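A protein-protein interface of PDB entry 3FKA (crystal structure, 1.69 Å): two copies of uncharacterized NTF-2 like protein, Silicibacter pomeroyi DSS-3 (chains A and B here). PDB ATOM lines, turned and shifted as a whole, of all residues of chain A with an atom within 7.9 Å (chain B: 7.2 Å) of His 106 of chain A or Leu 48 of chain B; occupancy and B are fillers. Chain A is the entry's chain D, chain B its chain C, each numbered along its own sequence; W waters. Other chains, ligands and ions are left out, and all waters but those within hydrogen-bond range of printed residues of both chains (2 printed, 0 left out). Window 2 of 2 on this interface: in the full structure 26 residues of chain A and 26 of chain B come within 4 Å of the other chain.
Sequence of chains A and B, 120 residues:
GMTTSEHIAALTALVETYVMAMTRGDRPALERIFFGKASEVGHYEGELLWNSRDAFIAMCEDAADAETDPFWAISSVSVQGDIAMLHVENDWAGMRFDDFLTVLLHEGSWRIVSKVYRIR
Printed residues of chain B within 4 Å of Lys 37 of chain A: Trp 50 (3.4 Å).
Printed residues of chain B within 4 Å of Leu 104 of chain A: His 43 (3.9 Å) and Leu 48 (3.3 Å).
Printed residues of chain B within 4 Å of His 106 of chain A: His 43 (2.9 Å) and Leu 48 (3.7 Å).
Of the printed residues of chain B, Val 113 of chain A touches Val 41 and Trp 50.
Of the printed residues of chain A, Val 41 of chain B touches Val 113 (3.7 Å).
Leu 48 of chain B touches three residues of chain A.
Printed residues of chain A within 4 Å of Trp 50 of chain B: Phe 35 (3.7 Å), Lys 37 (3.4 Å) and Val 113 (3.8 Å).
The nearest printed residue of chain A that does not touch Val 41 of chain B is Leu 104 of chain A (4.3 Å).
The side-chain carboxylate (OD2) of Asp 82 of chain A sits at hydrogen-bond distance from a ring nitrogen (ND1) of His 43 of chain B, at 2.7 Å.
NE2 of His 43 of chain B sits at hydrogen-bond distance from ND1 of His 106 of chain A (2.9 Å).
Leu 48 of chain B touches Phe 35 of chain A.
CZ3 of Trp 50 of chain B touches CG of Phe 35 of chain A, at 3.7 Å.
Lys 37 of chain A touches Trp 50 of chain B (CB to CZ2, 3.4 Å).
His 43 of chain B touches Leu 104 of chain A (CE1 to CG, 3.9 Å).
CD1 of Leu 48 of chain B touches CD2 of Leu 104 of chain A, 3.3 Å away.
O of Leu 105 of chain A touches CE1 of His 43 of chain B, 3.2 Å away.
CB of Leu 48 of chain B touches CE1 of His 106 of chain A, at 3.7 Å.
Val 41 of chain B touches Val 113 of chain A.
Val 113 of chain A touches Trp 50 of chain B.
Water W2 lies within hydrogen-bond range of O of Trp 50 of chain B (2.7 Å) and NZ of Lys 37 of chain A (2.8 Å).
Water W1 lies within hydrogen-bond range of the backbone carbonyl oxygen (O) of Tyr 117 of chain B, the side-chain carboxylate (OD1) of Asp 82 of chain A and the backbone NH (N) of His 43 of chain B.
Hydrophobic or aromatic side chains of chain A within 4 Å of the printed part of chain B: Phe 35, Leu 104, His 106 and Val 113.
Of the 12 printed residues of chain B, 4 touch a printed residue of chain A.
Hydrophobic or aromatic side chains of chain B that line the printed part of chain A: Val 41, His 43, Leu 48 and Trp 50.
Among the printed residues, no Asp or Glu carboxylate lies within 4 Å of a Lys or Arg side-chain nitrogen of the other chain.
No position is printed for both chains.
Of the 11 pairs that touch across the chains among the printed residues, none has its exchanged pair printed and touching as well.
O of Asp 82 of chain A sits at hydrogen-bond distance from N of Leu 105 of chain A (2.8 Å).
The backbone carbonyl oxygen of Arg 111 of chain A lies within hydrogen-bond range of the backbone NH of Leu 104 of chain A (2.9 Å).
The backbone NH of Tyr 117 of chain B lies within hydrogen-bond range of the backbone carbonyl oxygen of Val 41 of chain B, 3.0 Å away.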
ATOM      1  N   PHE A  35      19.744  23.337  23.966  1.00  0.00           N
ATOM      2  CA  PHE A  35      20.874  22.754  23.277  1.00  0.00           C
ATOM      3  C   PHE A  35      20.734  23.007  21.774  1.00  0.00           C
ATOM      4  O   PHE A  35      19.632  23.032  21.246  1.00  0.00           O
ATOM      5  CB  PHE A  35      20.974  21.235  23.458  1.00  0.00           C
ATOM      6  CG  PHE A  35      21.678  20.807  24.696  1.00  0.00           C
ATOM      7  CD1 PHE A  35      23.069  20.800  24.729  1.00  0.00           C
ATOM      8  CD2 PHE A  35      20.973  20.337  25.793  1.00  0.00           C
ATOM      9  CE1 PHE A  35      23.756  20.375  25.881  1.00  0.00           C
ATOM     10  CE2 PHE A  35      21.643  19.902  26.930  1.00  0.00           C
ATOM     11  CZ  PHE A  35      23.030  19.934  26.975  1.00  0.00           C
ATOM     12  N   LYS A  37      21.245  20.996  19.430  1.00  0.00           N
ATOM     13  CA  LYS A  37      20.662  19.798  18.808  1.00  0.00           C
ATOM     14  C   LYS A  37      19.219  19.539  19.224  1.00  0.00           C
ATOM     15  O   LYS A  37      18.591  18.608  18.710  1.00  0.00           O
ATOM     16  CB  LYS A  37      21.517  18.553  19.142  1.00  0.00           C
ATOM     17  CG  LYS A  37      22.917  18.574  18.586  1.00  0.00           C
ATOM     18  CD  LYS A  37      23.741  17.399  19.132  1.00  0.00           C
ATOM     19  CE  LYS A  37      25.181  17.493  18.771  1.00  0.00           C
ATOM     20  NZ  LYS A  37      26.040  16.504  19.532  1.00  0.00           N
ATOM     21  N   ASP A  82      20.800  14.625  37.340  1.00  0.00           N
ATOM     22  CA  ASP A  82      21.040  15.739  36.404  1.00  0.00           C
ATOM     23  C   ASP A  82      20.013  15.847  35.253  1.00  0.00           C
ATOM     24  O   ASP A  82      20.302  16.520  34.268  1.00  0.00           O
ATOM     25  CB  ASP A  82      22.490  15.700  35.866  1.00  0.00           C
ATOM     26  CG  ASP A  82      22.827  14.443  35.095  1.00  0.00           C
ATOM     27  OD1 ASP A  82      21.951  13.601  34.831  1.00  0.00           O
ATOM     28  OD2 ASP A  82      24.027  14.304  34.750  1.00  0.00           O
ATOM     29  N   VAL A 103      15.055  18.429  30.336  1.00  0.00           N
ATOM     30  CA  VAL A 103      16.205  19.246  30.557  1.00  0.00           C
ATOM     31  C   VAL A 103      17.368  18.457  31.161  1.00  0.00           C
ATOM     32  O   VAL A 103      17.150  17.484  31.867  1.00  0.00           O
ATOM     33  CB  VAL A 103      15.745  20.381  31.538  1.00  0.00           C
ATOM     34  CG1 VAL A 103      16.666  21.570  31.467  1.00  0.00           C
ATOM     35  CG2 VAL A 103      14.297  20.881  31.232  1.00  0.00           C
ATOM     36  N   LEU A 104      18.591  18.878  30.872  1.00  0.00           N
ATOM     37  CA  LEU A 104      19.788  18.222  31.382  1.00  0.00           C
ATOM     38  C   LEU A 104      20.705  19.263  32.013  1.00  0.00           C
ATOM     39  O   LEU A 104      20.894  20.326  31.423  1.00  0.00           O
ATOM     40  CB  LEU A 104      20.550  17.538  30.262  1.00  0.00           C
ATOM     41  CG  LEU A 104      21.845  16.753  30.547  1.00  0.00           C
ATOM     42  CD1 LEU A 104      21.524  15.468  31.249  1.00  0.00           C
ATOM     43  CD2 LEU A 104      22.626  16.485  29.268  1.00  0.00           C
ATOM     44  N   LEU A 105      21.233  18.959  33.208  1.00  0.00           N
ATOM     45  CA  LEU A 105      22.201  19.822  33.871  1.00  0.00           C
ATOM     46  C   LEU A 105      23.553  19.466  33.258  1.00  0.00           C
ATOM     47  O   LEU A 105      24.055  18.381  33.500  1.00  0.00           O
ATOM     48  CB  LEU A 105      22.202  19.603  35.376  1.00  0.00           C
ATOM     49  CG  LEU A 105      23.195  20.430  36.197  1.00  0.00           C
ATOM     50  CD1 LEU A 105      22.913  21.934  36.096  1.00  0.00           C
ATOM     51  CD2 LEU A 105      23.118  19.947  37.616  1.00  0.00           C
ATOM     52  N   HIS A 106      24.145  20.375  32.479  1.00  0.00           N
ATOM     53  CA  HIS A 106      25.410  20.114  31.809  1.00  0.00           C
ATOM     54  C   HIS A 106      26.331  21.297  31.980  1.00  0.00           C
ATOM     55  O   HIS A 106      25.951  22.409  31.630  1.00  0.00           O
ATOM     56  CB  HIS A 106      25.182  19.848  30.312  1.00  0.00           C
ATOM     57  CG  HIS A 106      26.439  19.534  29.557  1.00  0.00           C
ATOM     58  ND1 HIS A 106      27.119  18.343  29.711  1.00  0.00           N
ATOM     59  CD2 HIS A 106      27.141  20.252  28.647  1.00  0.00           C
ATOM     60  CE1 HIS A 106      28.194  18.346  28.938  1.00  0.00           C
ATOM     61  NE2 HIS A 106      28.230  19.496  28.284  1.00  0.00           N
ATOM     62  N   GLU A 107      27.512  21.026  32.538  1.00  0.00           N
ATOM     63  CA  GLU A 107      28.552  22.021  32.818  1.00  0.00           C
ATOM     64  C   GLU A 107      27.999  23.253  33.542  1.00  0.00           C
ATOM     65  O   GLU A 107      28.124  24.412  33.104  1.00  0.00           O
ATOM     66  CB  GLU A 107      29.312  22.362  31.545  1.00  0.00           C
ATOM     67  CG  GLU A 107      30.061  21.138  31.028  1.00  0.00           C
ATOM     68  CD  GLU A 107      30.933  21.422  29.836  1.00  0.00           C
ATOM     69  OE1 GLU A 107      31.092  22.598  29.454  1.00  0.00           O
ATOM     70  OE2 GLU A 107      31.467  20.450  29.275  1.00  0.00           O
ATOM     71  N   GLY A 108      27.369  22.957  34.672  1.00  0.00           N
ATOM     72  CA  GLY A 108      26.814  23.968  35.552  1.00  0.00           C
ATOM     73  C   GLY A 108      25.438  24.551  35.352  1.00  0.00           C
ATOM     74  O   GLY A 108      24.932  25.172  36.290  1.00  0.00           O
ATOM     75  N   SER A 109      24.823  24.383  34.177  1.00  0.00           N
ATOM     76  CA  SER A 109      23.486  24.952  33.954  1.00  0.00           C
ATOM     77  C   SER A 109      22.531  24.002  33.246  1.00  0.00           C
ATOM     78  O   SER A 109      22.938  23.128  32.495  1.00  0.00           O
ATOM     79  CB  SER A 109      23.578  26.256  33.166  1.00  0.00           C
ATOM     80  OG  SER A 109      24.069  26.042  31.861  1.00  0.00           O
ATOM     81  N   TRP A 110      21.253  24.207  33.529  1.00  0.00           N
ATOM     82  CA  TRP A 110      20.185  23.429  32.937  1.00  0.00           C
ATOM     83  C   TRP A 110      19.896  23.904  31.512  1.00  0.00           C
ATOM     84  O   TRP A 110      19.737  25.110  31.284  1.00  0.00           O
ATOM     85  CB  TRP A 110      18.927  23.536  33.798  1.00  0.00           C
ATOM     86  CG  TRP A 110      19.048  22.868  35.142  1.00  0.00           C
ATOM     87  CD1 TRP A 110      19.406  23.442  36.325  1.00  0.00           C
ATOM     88  CD2 TRP A 110      18.817  21.484  35.425  1.00  0.00           C
ATOM     89  NE1 TRP A 110      19.399  22.508  37.326  1.00  0.00           N
ATOM     90  CE2 TRP A 110      19.037  21.296  36.811  1.00  0.00           C
ATOM     91  CE3 TRP A 110      18.429  20.388  34.652  1.00  0.00           C
ATOM     92  CZ2 TRP A 110      18.901  20.042  37.432  1.00  0.00           C
ATOM     93  CZ3 TRP A 110      18.290  19.142  35.270  1.00  0.00           C
ATOM     94  CH2 TRP A 110      18.527  18.981  36.644  1.00  0.00           C
ATOM     95  N   ARG A 111      19.897  22.960  30.568  1.00  0.00           N
ATOM     96  CA  ARG A 111      19.586  23.236  29.164  1.00  0.00           C
ATOM     97  C   ARG A 111      18.530  22.263  28.664  1.00  0.00           C
ATOM     98  O   ARG A 111      18.568  21.061  28.957  1.00  0.00           O
ATOM     99  CB  ARG A 111      20.820  23.176  28.258  1.00  0.00           C
ATOM    100  CG  ARG A 111      21.744  24.370  28.324  1.00  0.00           C
ATOM    101  CD  ARG A 111      22.949  24.170  27.382  1.00  0.00           C
ATOM    102  NE  ARG A 111      23.778  25.375  27.320  1.00  0.00           N
ATOM    103  CZ  ARG A 111      23.772  26.309  26.360  1.00  0.00           C
ATOM    104  NH1 ARG A 111      23.011  26.215  25.267  1.00  0.00           N
ATOM    105  NH2 ARG A 111      24.579  27.363  26.491  1.00  0.00           N
ATOM    106  N   VAL A 113      16.720  19.806  26.336  1.00  0.00           N
ATOM    107  CA  VAL A 113      17.069  18.781  25.355  1.00  0.00           C
ATOM    108  C   VAL A 113      15.963  18.575  24.333  1.00  0.00           C
ATOM    109  O   VAL A 113      16.225  18.384  23.135  1.00  0.00           O
ATOM    110  CB  VAL A 113      17.366  17.437  26.080  1.00  0.00           C
ATOM    111  CG1 VAL A 113      17.461  16.236  25.101  1.00  0.00           C
ATOM    112  CG2 VAL A 113      18.625  17.574  26.914  1.00  0.00           C
ATOM    113  N   VAL B  41      19.683  11.035  24.988  1.00  0.00           N
ATOM    114  CA  VAL B  41      20.680  11.938  25.542  1.00  0.00           C
ATOM    115  C   VAL B  41      20.946  11.731  27.028  1.00  0.00           C
ATOM    116  O   VAL B  41      20.010  11.575  27.796  1.00  0.00           O
ATOM    117  CB  VAL B  41      20.200  13.387  25.369  1.00  0.00           C
ATOM    118  CG1 VAL B  41      21.287  14.365  25.813  1.00  0.00           C
ATOM    119  CG2 VAL B  41      19.803  13.676  23.914  1.00  0.00           C
ATOM    120  N   GLY B  42      22.214  11.731  27.425  1.00  0.00           N
ATOM    121  CA  GLY B  42      22.579  11.580  28.846  1.00  0.00           C
ATOM    122  C   GLY B  42      24.077  11.609  29.046  1.00  0.00           C
ATOM    123  O   GLY B  42      24.832  11.623  28.068  1.00  0.00           O
ATOM    124  N   HIS B  43      24.510  11.679  30.310  1.00  0.00           N
ATOM    125  CA  HIS B  43      25.930  11.633  30.624  1.00  0.00           C
ATOM    126  C   HIS B  43      26.302  10.173  30.806  1.00  0.00           C
ATOM    127  O   HIS B  43      25.598   9.421  31.490  1.00  0.00           O
ATOM    128  CB  HIS B  43      26.316  12.419  31.860  1.00  0.00           C
ATOM    129  CG  HIS B  43      26.168  13.888  31.689  1.00  0.00           C
ATOM    130  ND1 HIS B  43      25.253  14.628  32.399  1.00  0.00           N
ATOM    131  CD2 HIS B  43      26.796  14.750  30.859  1.00  0.00           C
ATOM    132  CE1 HIS B  43      25.346  15.894  32.032  1.00  0.00           C
ATOM    133  NE2 HIS B  43      26.265  15.993  31.089  1.00  0.00           N
ATOM    134  N   TYR B  44      27.411   9.786  30.192  1.00  0.00           N
ATOM    135  CA  TYR B  44      27.887   8.425  30.243  1.00  0.00           C
ATOM    136  C   TYR B  44      29.385   8.543  30.425  1.00  0.00           C
ATOM    137  O   TYR B  44      30.078   9.131  29.581  1.00  0.00           O
ATOM    138  CB  TYR B  44      27.486   7.706  28.957  1.00  0.00           C
ATOM    139  CG  TYR B  44      27.774   6.225  28.936  1.00  0.00           C
ATOM    140  CD1 TYR B  44      26.897   5.330  29.539  1.00  0.00           C
ATOM    141  CD2 TYR B  44      28.888   5.713  28.272  1.00  0.00           C
ATOM    142  CE1 TYR B  44      27.137   3.967  29.521  1.00  0.00           C
ATOM    143  CE2 TYR B  44      29.145   4.343  28.248  1.00  0.00           C
ATOM    144  CZ  TYR B  44      28.258   3.473  28.878  1.00  0.00           C
ATOM    145  OH  TYR B  44      28.482   2.112  28.870  1.00  0.00           O
ATOM    146  N   GLU B  45      29.870   7.994  31.541  1.00  0.00           N
ATOM    147  CA  GLU B  45      31.286   8.025  31.959  1.00  0.00           C
ATOM    148  C   GLU B  45      31.914   9.433  31.783  1.00  0.00           C
ATOM    149  O   GLU B  45      32.931   9.626  31.115  1.00  0.00           O
ATOM    150  CB  GLU B  45      32.087   6.836  31.355  1.00  0.00           C
ATOM    151  CG  GLU B  45      31.992   6.593  29.839  1.00  0.00           C
ATOM    152  CD  GLU B  45      32.563   5.237  29.376  1.00  0.00           C
ATOM    153  OE1 GLU B  45      32.967   4.400  30.225  1.00  0.00           O
ATOM    154  OE2 GLU B  45      32.585   5.006  28.137  1.00  0.00           O
ATOM    155  N   GLY B  46      31.226  10.398  32.397  1.00  0.00           N
ATOM    156  CA  GLY B  46      31.611  11.798  32.432  1.00  0.00           C
ATOM    157  C   GLY B  46      31.388  12.700  31.231  1.00  0.00           C
ATOM    158  O   GLY B  46      31.646  13.896  31.328  1.00  0.00           O
ATOM    159  N   GLU B  47      30.894  12.160  30.123  1.00  0.00           N
ATOM    160  CA  GLU B  47      30.693  12.942  28.917  1.00  0.00           C
ATOM    161  C   GLU B  47      29.264  12.907  28.469  1.00  0.00           C
ATOM    162  O   GLU B  47      28.544  11.969  28.774  1.00  0.00           O
ATOM    163  CB  GLU B  47      31.567  12.366  27.820  1.00  0.00           C
ATOM    164  CG  GLU B  47      33.031  12.360  28.192  1.00  0.00           C
ATOM    165  CD  GLU B  47      33.902  11.710  27.155  1.00  0.00           C
ATOM    166  OE1 GLU B  47      33.377  11.197  26.137  1.00  0.00           O
ATOM    167  OE2 GLU B  47      35.123  11.692  27.384  1.00  0.00           O
ATOM    168  N   LEU B  48      28.874  13.930  27.720  1.00  0.00           N
ATOM    169  CA  LEU B  48      27.543  14.027  27.188  1.00  0.00           C
ATOM    170  C   LEU B  48      27.475  13.148  25.947  1.00  0.00           C
ATOM    171  O   LEU B  48      28.325  13.275  25.055  1.00  0.00           O
ATOM    172  CB  LEU B  48      27.211  15.476  26.802  1.00  0.00           C
ATOM    173  CG  LEU B  48      25.840  15.743  26.153  1.00  0.00           C
ATOM    174  CD1 LEU B  48      24.727  15.243  27.032  1.00  0.00           C
ATOM    175  CD2 LEU B  48      25.674  17.228  25.866  1.00  0.00           C
ATOM    176  N   LEU B  49      26.522  12.225  25.914  1.00  0.00           N
ATOM    177  CA  LEU B  49      26.312  11.360  24.764  1.00  0.00           C
ATOM    178  C   LEU B  49      24.964  11.752  24.176  1.00  0.00           C
ATOM    179  O   LEU B  49      23.961  11.706  24.871  1.00  0.00           O
ATOM    180  CB  LEU B  49      26.361   9.893  25.166  1.00  0.00           C
ATOM    181  CG  LEU B  49      26.308   8.810  24.093  1.00  0.00           C
ATOM    182  CD1 LEU B  49      27.317   9.028  22.973  1.00  0.00           C
ATOM    183  CD2 LEU B  49      26.530   7.456  24.775  1.00  0.00           C
ATOM    184  N   TRP B  50      24.966  12.180  22.918  1.00  0.00           N
ATOM    185  CA  TRP B  50      23.773  12.584  22.210  1.00  0.00           C
ATOM    186  C   TRP B  50      23.651  11.658  20.998  1.00  0.00           C
ATOM    187  O   TRP B  50      24.292  11.897  19.968  1.00  0.00           O
ATOM    188  CB  TRP B  50      23.867  14.053  21.758  1.00  0.00           C
ATOM    189  CG  TRP B  50      22.534  14.570  21.286  1.00  0.00           C
ATOM    190  CD1 TRP B  50      21.801  14.143  20.208  1.00  0.00           C
ATOM    191  CD2 TRP B  50      21.814  15.655  21.843  1.00  0.00           C
ATOM    192  NE1 TRP B  50      20.640  14.848  20.117  1.00  0.00           N
ATOM    193  CE2 TRP B  50      20.629  15.799  21.098  1.00  0.00           C
ATOM    194  CE3 TRP B  50      22.035  16.510  22.931  1.00  0.00           C
ATOM    195  CZ2 TRP B  50      19.676  16.764  21.401  1.00  0.00           C
ATOM    196  CZ3 TRP B  50      21.080  17.463  23.219  1.00  0.00           C
ATOM    197  CH2 TRP B  50      19.920  17.574  22.461  1.00  0.00           C
ATOM    198  N   ASN B  51      22.825  10.622  21.124  1.00  0.00           N
ATOM    199  CA  ASN B  51      22.623   9.627  20.075  1.00  0.00           C
ATOM    200  C   ASN B  51      21.413   9.821  19.217  1.00  0.00           C
ATOM    201  O   ASN B  51      20.361  10.177  19.723  1.00  0.00           O
ATOM    202  CB  ASN B  51      22.425   8.232  20.705  1.00  0.00           C
ATOM    203  CG  ASN B  51      23.655   7.719  21.404  1.00  0.00           C
ATOM    204  OD1 ASN B  51      24.759   7.881  20.917  1.00  0.00           O
ATOM    205  ND2 ASN B  51      23.457   7.028  22.530  1.00  0.00           N
ATOM    206  N   TYR B 117      18.323  10.398  29.934  1.00  0.00           N
ATOM    207  CA  TYR B 117      18.552   9.512  31.068  1.00  0.00           C
ATOM    208  C   TYR B 117      19.673   9.909  31.975  1.00  0.00           C
ATOM    209  O   TYR B 117      20.514  10.729  31.606  1.00  0.00           O
ATOM    210  CB  TYR B 117      18.920   8.105  30.519  1.00  0.00           C
ATOM    211  CG  TYR B 117      20.251   8.079  29.760  1.00  0.00           C
ATOM    212  CD1 TYR B 117      21.463   7.864  30.422  1.00  0.00           C
ATOM    213  CD2 TYR B 117      20.301   8.299  28.390  1.00  0.00           C
ATOM    214  CE1 TYR B 117      22.686   7.865  29.749  1.00  0.00           C
ATOM    215  CE2 TYR B 117      21.518   8.304  27.705  1.00  0.00           C
ATOM    216  CZ  TYR B 117      22.704   8.077  28.381  1.00  0.00           C
ATOM    217  OH  TYR B 117      23.910   8.073  27.717  1.00  0.00           O
HETATM  218  O   HOH W   1      22.666  12.076  32.634  1.00  0.00           O
HETATM  219  O   HOH W   2      25.358  13.961  18.603  1.00  0.00           O
